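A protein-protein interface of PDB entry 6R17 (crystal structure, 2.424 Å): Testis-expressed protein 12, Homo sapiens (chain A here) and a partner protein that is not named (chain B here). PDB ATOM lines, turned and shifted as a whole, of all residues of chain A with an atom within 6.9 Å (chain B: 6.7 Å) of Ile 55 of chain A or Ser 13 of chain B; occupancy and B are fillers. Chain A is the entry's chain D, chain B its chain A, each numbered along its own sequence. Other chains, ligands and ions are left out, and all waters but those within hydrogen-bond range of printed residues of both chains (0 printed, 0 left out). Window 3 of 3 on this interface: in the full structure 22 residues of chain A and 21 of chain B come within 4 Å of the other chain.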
ATOM      1  N   LYS A  50     -22.046 -24.576 -10.339  1.00  0.00           N
ATOM      2  CA  LYS A  50     -21.344 -24.309 -11.592  1.00  0.00           C
ATOM      3  C   LYS A  50     -21.030 -22.827 -11.734  1.00  0.00           C
ATOM      4  O   LYS A  50     -19.910 -22.447 -12.111  1.00  0.00           O
ATOM      5  CB  LYS A  50     -22.176 -24.781 -12.783  1.00  0.00           C
ATOM      6  CG  LYS A  50     -22.434 -26.269 -12.824  1.00  0.00           C
ATOM      7  CD  LYS A  50     -21.163 -27.050 -12.553  1.00  0.00           C
ATOM      8  CE  LYS A  50     -21.293 -28.479 -13.041  1.00  0.00           C
ATOM      9  NZ  LYS A  50     -22.721 -28.882 -13.165  1.00  0.00           N
ATOM     10  N   GLU A  51     -22.013 -21.973 -11.440  1.00  0.00           N
ATOM     11  CA  GLU A  51     -21.778 -20.532 -11.546  1.00  0.00           C
ATOM     12  C   GLU A  51     -20.678 -20.081 -10.589  1.00  0.00           C
ATOM     13  O   GLU A  51     -19.806 -19.272 -10.956  1.00  0.00           O
ATOM     14  CB  GLU A  51     -23.073 -19.769 -11.279  1.00  0.00           C
ATOM     15  CG  GLU A  51     -23.308 -18.613 -12.232  1.00  0.00           C
ATOM     16  CD  GLU A  51     -24.703 -18.037 -12.110  1.00  0.00           C
ATOM     17  OE1 GLU A  51     -24.857 -16.970 -11.479  1.00  0.00           O
ATOM     18  OE2 GLU A  51     -25.652 -18.662 -12.632  1.00  0.00           O
ATOM     19  N   ALA A  52     -20.702 -20.598  -9.357  1.00  0.00           N
ATOM     20  CA  ALA A  52     -19.669 -20.251  -8.385  1.00  0.00           C
ATOM     21  C   ALA A  52     -18.286 -20.635  -8.895  1.00  0.00           C
ATOM     22  O   ALA A  52     -17.337 -19.843  -8.817  1.00  0.00           O
ATOM     23  CB  ALA A  52     -19.959 -20.936  -7.052  1.00  0.00           C
ATOM     24  N   ASN A  53     -18.153 -21.852  -9.427  1.00  0.00           N
ATOM     25  CA  ASN A  53     -16.852 -22.295  -9.915  1.00  0.00           C
ATOM     26  C   ASN A  53     -16.378 -21.450 -11.094  1.00  0.00           C
ATOM     27  O   ASN A  53     -15.179 -21.180 -11.225  1.00  0.00           O
ATOM     28  CB  ASN A  53     -16.893 -23.779 -10.268  1.00  0.00           C
ATOM     29  CG  ASN A  53     -15.507 -24.378 -10.429  1.00  0.00           C
ATOM     30  OD1 ASN A  53     -14.586 -24.073  -9.661  1.00  0.00           O
ATOM     31  ND2 ASN A  53     -15.359 -25.259 -11.413  1.00  0.00           N
ATOM     32  N   ALA A  54     -17.293 -21.046 -11.980  1.00  0.00           N
ATOM     33  CA  ALA A  54     -16.894 -20.181 -13.091  1.00  0.00           C
ATOM     34  C   ALA A  54     -16.344 -18.848 -12.587  1.00  0.00           C
ATOM     35  O   ALA A  54     -15.294 -18.371 -13.056  1.00  0.00           O
ATOM     36  CB  ALA A  54     -18.074 -19.950 -14.034  1.00  0.00           C
ATOM     37  N   ILE A  55     -17.043 -18.227 -11.629  1.00  0.00           N
ATOM     38  CA  ILE A  55     -16.553 -16.965 -11.073  1.00  0.00           C
ATOM     39  C   ILE A  55     -15.189 -17.161 -10.423  1.00  0.00           C
ATOM     40  O   ILE A  55     -14.275 -16.344 -10.598  1.00  0.00           O
ATOM     41  CB  ILE A  55     -17.571 -16.372 -10.081  1.00  0.00           C
ATOM     42  CG1 ILE A  55     -18.857 -15.978 -10.805  1.00  0.00           C
ATOM     43  CG2 ILE A  55     -16.974 -15.173  -9.347  1.00  0.00           C
ATOM     44  CD1 ILE A  55     -20.002 -15.673  -9.872  1.00  0.00           C
ATOM     45  N   GLU A  56     -15.025 -18.262  -9.688  1.00  0.00           N
ATOM     46  CA  GLU A  56     -13.749 -18.535  -9.032  1.00  0.00           C
ATOM     47  C   GLU A  56     -12.629 -18.715 -10.051  1.00  0.00           C
ATOM     48  O   GLU A  56     -11.505 -18.245  -9.838  1.00  0.00           O
ATOM     49  CB  GLU A  56     -13.878 -19.780  -8.156  1.00  0.00           C
ATOM     50  CG  GLU A  56     -12.558 -20.372  -7.703  1.00  0.00           C
ATOM     51  CD  GLU A  56     -12.656 -21.864  -7.466  1.00  0.00           C
ATOM     52  OE1 GLU A  56     -12.228 -22.634  -8.351  1.00  0.00           O
ATOM     53  OE2 GLU A  56     -13.180 -22.269  -6.408  1.00  0.00           O
ATOM     54  N   ASN A  57     -12.911 -19.419 -11.152  1.00  0.00           N
ATOM     55  CA  ASN A  57     -11.901 -19.624 -12.185  1.00  0.00           C
ATOM     56  C   ASN A  57     -11.461 -18.310 -12.804  1.00  0.00           C
ATOM     57  O   ASN A  57     -10.260 -18.082 -12.999  1.00  0.00           O
ATOM     58  CB  ASN A  57     -12.434 -20.559 -13.267  1.00  0.00           C
ATOM     59  CG  ASN A  57     -12.376 -22.008 -12.855  1.00  0.00           C
ATOM     60  OD1 ASN A  57     -11.797 -22.347 -11.824  1.00  0.00           O
ATOM     61  ND2 ASN A  57     -12.981 -22.875 -13.657  1.00  0.00           N
ATOM     62  N   PHE A  58     -12.411 -17.428 -13.125  1.00  0.00           N
ATOM     63  CA  PHE A  58     -11.986 -16.144 -13.673  1.00  0.00           C
ATOM     64  C   PHE A  58     -11.195 -15.350 -12.638  1.00  0.00           C
ATOM     65  O   PHE A  58     -10.204 -14.695 -12.979  1.00  0.00           O
ATOM     66  CB  PHE A  58     -13.164 -15.325 -14.191  1.00  0.00           C
ATOM     67  CG  PHE A  58     -12.740 -14.084 -14.941  1.00  0.00           C
ATOM     68  CD1 PHE A  58     -12.177 -14.200 -16.205  1.00  0.00           C
ATOM     69  CD2 PHE A  58     -12.889 -12.817 -14.397  1.00  0.00           C
ATOM     70  CE1 PHE A  58     -11.778 -13.084 -16.916  1.00  0.00           C
ATOM     71  CE2 PHE A  58     -12.490 -11.691 -15.110  1.00  0.00           C
ATOM     72  CZ  PHE A  58     -11.934 -11.829 -16.371  1.00  0.00           C
ATOM     73  N   LEU A  59     -11.619 -15.383 -11.369  1.00  0.00           N
ATOM     74  CA  LEU A  59     -10.897 -14.626 -10.346  1.00  0.00           C
ATOM     75  C   LEU A  59      -9.486 -15.159 -10.139  1.00  0.00           C
ATOM     76  O   LEU A  59      -8.585 -14.386  -9.794  1.00  0.00           O
ATOM     77  CB  LEU A  59     -11.662 -14.639  -9.019  1.00  0.00           C
ATOM     78  CG  LEU A  59     -12.982 -13.875  -9.015  1.00  0.00           C
ATOM     79  CD1 LEU A  59     -13.648 -13.886  -7.638  1.00  0.00           C
ATOM     80  CD2 LEU A  59     -12.715 -12.453  -9.477  1.00  0.00           C
ATOM     81  N   ILE A  60      -9.271 -16.464 -10.320  1.00  0.00           N
ATOM     82  CA  ILE A  60      -7.935 -17.018 -10.126  1.00  0.00           C
ATOM     83  C   ILE A  60      -6.982 -16.452 -11.165  1.00  0.00           C
ATOM     84  O   ILE A  60      -5.865 -16.033 -10.838  1.00  0.00           O
ATOM     85  CB  ILE A  60      -7.997 -18.559 -10.178  1.00  0.00           C
ATOM     86  CG1 ILE A  60      -8.496 -19.114  -8.839  1.00  0.00           C
ATOM     87  CG2 ILE A  60      -6.650 -19.159 -10.576  1.00  0.00           C
ATOM     88  CD1 ILE A  60      -8.707 -20.625  -8.822  1.00  0.00           C
ATOM     89  N   SER B   8     -17.116  -4.870  -9.406  1.00  0.00           N
ATOM     90  CA  SER B   8     -18.512  -4.642  -9.044  1.00  0.00           C
ATOM     91  C   SER B   8     -19.468  -5.510  -9.862  1.00  0.00           C
ATOM     92  O   SER B   8     -20.508  -5.936  -9.347  1.00  0.00           O
ATOM     93  CB  SER B   8     -18.863  -3.165  -9.211  1.00  0.00           C
ATOM     94  OG  SER B   8     -18.738  -2.767 -10.563  1.00  0.00           O
ATOM     95  N   SER B   9     -19.153  -5.765 -11.135  1.00  0.00           N
ATOM     96  CA  SER B   9     -19.983  -6.666 -11.933  1.00  0.00           C
ATOM     97  C   SER B   9     -19.976  -8.073 -11.342  1.00  0.00           C
ATOM     98  O   SER B   9     -21.035  -8.689 -11.132  1.00  0.00           O
ATOM     99  CB  SER B   9     -19.487  -6.676 -13.381  1.00  0.00           C
ATOM    100  OG  SER B   9     -20.056  -7.743 -14.119  1.00  0.00           O
ATOM    101  N   LEU B  10     -18.787  -8.587 -11.027  1.00  0.00           N
ATOM    102  CA  LEU B  10     -18.746  -9.892 -10.377  1.00  0.00           C
ATOM    103  C   LEU B  10     -19.338  -9.821  -8.972  1.00  0.00           C
ATOM    104  O   LEU B  10     -19.780 -10.843  -8.446  1.00  0.00           O
ATOM    105  CB  LEU B  10     -17.324 -10.459 -10.367  1.00  0.00           C
ATOM    106  CG  LEU B  10     -16.178  -9.734  -9.678  1.00  0.00           C
ATOM    107  CD1 LEU B  10     -15.941 -10.334  -8.306  1.00  0.00           C
ATOM    108  CD2 LEU B  10     -14.919  -9.805 -10.532  1.00  0.00           C
ATOM    109  N   ASP B  11     -19.342  -8.638  -8.352  1.00  0.00           N
ATOM    110  CA  ASP B  11     -20.004  -8.467  -7.062  1.00  0.00           C
ATOM    111  C   ASP B  11     -21.504  -8.640  -7.182  1.00  0.00           C
ATOM    112  O   ASP B  11     -22.143  -9.226  -6.302  1.00  0.00           O
ATOM    113  CB  ASP B  11     -19.692  -7.091  -6.488  1.00  0.00           C
ATOM    114  CG  ASP B  11     -18.297  -7.003  -6.032  1.00  0.00           C
ATOM    115  OD1 ASP B  11     -17.789  -8.098  -5.756  1.00  0.00           O
ATOM    116  OD2 ASP B  11     -17.725  -5.896  -5.950  1.00  0.00           O
ATOM    117  N   SER B  12     -22.088  -8.106  -8.249  1.00  0.00           N
ATOM    118  CA  SER B  12     -23.504  -8.340  -8.487  1.00  0.00           C
ATOM    119  C   SER B  12     -23.751  -9.814  -8.754  1.00  0.00           C
ATOM    120  O   SER B  12     -24.765 -10.372  -8.320  1.00  0.00           O
ATOM    121  CB  SER B  12     -23.995  -7.485  -9.648  1.00  0.00           C
ATOM    122  OG  SER B  12     -23.907  -6.121  -9.302  1.00  0.00           O
ATOM    123  N   SER B  13     -22.813 -10.467  -9.443  1.00  0.00           N
ATOM    124  CA  SER B  13     -22.917 -11.914  -9.620  1.00  0.00           C
ATOM    125  C   SER B  13     -22.912 -12.639  -8.274  1.00  0.00           C
ATOM    126  O   SER B  13     -23.697 -13.569  -8.058  1.00  0.00           O
ATOM    127  CB  SER B  13     -21.775 -12.418 -10.501  1.00  0.00           C
ATOM    128  OG  SER B  13     -21.936 -11.982 -11.839  1.00  0.00           O
ATOM    129  N   ILE B  14     -22.032 -12.221  -7.360  1.00  0.00           N
ATOM    130  CA  ILE B  14     -21.955 -12.827  -6.031  1.00  0.00           C
ATOM    131  C   ILE B  14     -23.250 -12.601  -5.255  1.00  0.00           C
ATOM    132  O   ILE B  14     -23.771 -13.518  -4.598  1.00  0.00           O
ATOM    133  CB  ILE B  14     -20.739 -12.271  -5.265  1.00  0.00           C
ATOM    134  CG1 ILE B  14     -19.430 -12.727  -5.915  1.00  0.00           C
ATOM    135  CG2 ILE B  14     -20.786 -12.675  -3.799  1.00  0.00           C
ATOM    136  CD1 ILE B  14     -18.199 -12.050  -5.343  1.00  0.00           C
ATOM    137  N   ASP B  15     -23.788 -11.379  -5.321  1.00  0.00           N
ATOM    138  CA  ASP B  15     -25.035 -11.080  -4.627  1.00  0.00           C
ATOM    139  C   ASP B  15     -26.155 -11.958  -5.155  1.00  0.00           C
ATOM    140  O   ASP B  15     -26.917 -12.557  -4.384  1.00  0.00           O
ATOM    141  CB  ASP B  15     -25.411  -9.605  -4.811  1.00  0.00           C
ATOM    142  CG  ASP B  15     -24.451  -8.655  -4.129  1.00  0.00           C
ATOM    143  OD1 ASP B  15     -23.357  -9.093  -3.720  1.00  0.00           O
ATOM    144  OD2 ASP B  15     -24.799  -7.461  -3.999  1.00  0.00           O
ATOM    145  N   ILE B  16     -26.254 -12.058  -6.481  1.00  0.00           N
ATOM    146  CA  ILE B  16     -27.297 -12.871  -7.092  1.00  0.00           C
ATOM    147  C   ILE B  16     -27.130 -14.340  -6.723  1.00  0.00           C
ATOM    148  O   ILE B  16     -28.112 -15.023  -6.438  1.00  0.00           O
ATOM    149  CB  ILE B  16     -27.320 -12.646  -8.615  1.00  0.00           C
ATOM    150  CG1 ILE B  16     -27.662 -11.185  -8.917  1.00  0.00           C
ATOM    151  CG2 ILE B  16     -28.344 -13.539  -9.272  1.00  0.00           C
ATOM    152  CD1 ILE B  16     -29.073 -10.798  -8.531  1.00  0.00           C
ATOM    153  N   LEU B  17     -25.892 -14.845  -6.678  1.00  0.00           N
ATOM    154  CA  LEU B  17     -25.690 -16.252  -6.323  1.00  0.00           C
ATOM    155  C   LEU B  17     -26.113 -16.546  -4.888  1.00  0.00           C
ATOM    156  O   LEU B  17     -26.845 -17.512  -4.628  1.00  0.00           O
ATOM    157  CB  LEU B  17     -24.229 -16.654  -6.535  1.00  0.00           C
ATOM    158  CG  LEU B  17     -23.830 -17.134  -7.928  1.00  0.00           C
ATOM    159  CD1 LEU B  17     -22.365 -17.529  -7.938  1.00  0.00           C
ATOM    160  CD2 LEU B  17     -24.703 -18.309  -8.342  1.00  0.00           C
ATOM    161  N   GLN B  18     -25.658 -15.727  -3.937  1.00  0.00           N
ATOM    162  CA  GLN B  18     -26.027 -15.966  -2.541  1.00  0.00           C
ATOM    163  C   GLN B  18     -27.537 -15.841  -2.338  1.00  0.00           C
ATOM    164  O   GLN B  18     -28.161 -16.662  -1.642  1.00  0.00           O
ATOM    165  CB  GLN B  18     -25.252 -15.016  -1.626  1.00  0.00           C
ATOM    166  CG  GLN B  18     -23.815 -15.478  -1.351  1.00  0.00           C
ATOM    167  CD  GLN B  18     -22.978 -14.438  -0.625  1.00  0.00           C
ATOM    168  OE1 GLN B  18     -23.261 -13.242  -0.687  1.00  0.00           O
ATOM    169  NE2 GLN B  18     -21.940 -14.894   0.071  1.00  0.00           N
ATOM    170  N   ARG B  20     -29.910 -16.174  -4.613  1.00  0.00           N
ATOM    171  CA  ARG B  20     -30.531 -17.324  -5.257  1.00  0.00           C
ATOM    172  C   ARG B  20     -30.463 -18.544  -4.360  1.00  0.00           C
ATOM    173  O   ARG B  20     -31.393 -19.353  -4.335  1.00  0.00           O
ATOM    174  CB  ARG B  20     -29.850 -17.634  -6.588  1.00  0.00           C
ATOM    175  CG  ARG B  20     -30.189 -16.719  -7.744  1.00  0.00           C
ATOM    176  CD  ARG B  20     -29.139 -16.878  -8.833  1.00  0.00           C
ATOM    177  NE  ARG B  20     -29.221 -18.185  -9.503  1.00  0.00           N
ATOM    178  CZ  ARG B  20     -28.393 -18.577 -10.468  1.00  0.00           C
ATOM    179  NH1 ARG B  20     -27.405 -17.778 -10.857  1.00  0.00           N
ATOM    180  NH2 ARG B  20     -28.534 -19.768 -11.019  1.00  0.00           N
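NH1 of Arg 20 of chain B lies within salt-bridge range of OE2 of Glu 51 of chain A.
The backbone carbonyl oxygen (O) of Ser 9 of chain B is in hydrogen-bond range of the side-chain hydroxyl (OG) of Ser 13 of chain B, at 3.5 Å.
Among the printed residues, pairs that only touch across the chains: Glu 51 of chain A with Leu 17 of chain B (3.4 Å), Ala 52 of chain A with Leu 17 of chain B (3.8 Å), Ile 55 of chain A with Ser 13 of chain B (3.8 Å), Ile 55 of chain A with Leu 17 of chain B (3.6 Å) and Leu 59 of chain A with Leu 10 of chain B (3.6 Å).
Ile 55 of chain A touches two residues of chain B. Ser 13 of chain B touches one residue of chain A. Of the printed residues of chain A, Arg 20 of chain B touches Glu 51. Printed residues of chain A within 4 Å of Leu 10 of chain B: Leu 59. Printed residues of chain B within 4 Å of Leu 59 of chain A: Leu 10 (3.6 Å). Printed residues of chain B within 4 Å of Ala 52 of chain A: Leu 17. Ile 16 of chain B touches none of the printed residues of chain A. Asp 11 of chain B touches none of the printed residues of chain A. The nearest residue of chain B that does not touch Ile 55 of chain A is Ile 14 of chain B (4.7 Å). The nearest printed residue of chain B that does not touch Glu 51 of chain A is Ser 13 of chain B (5.0 Å).
Of the 11 printed residues of chain A, 4 touch a printed residue of chain B. Hydrophobic or aromatic side chains of chain B that line the printed part of chain A: Leu 10 and Leu 17. Among the printed residues, Asp or Glu carboxylates within 4 Å of a Lys or Arg side-chain nitrogen of the other chain: Glu 51 of chain A with Arg 20 of chain B.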
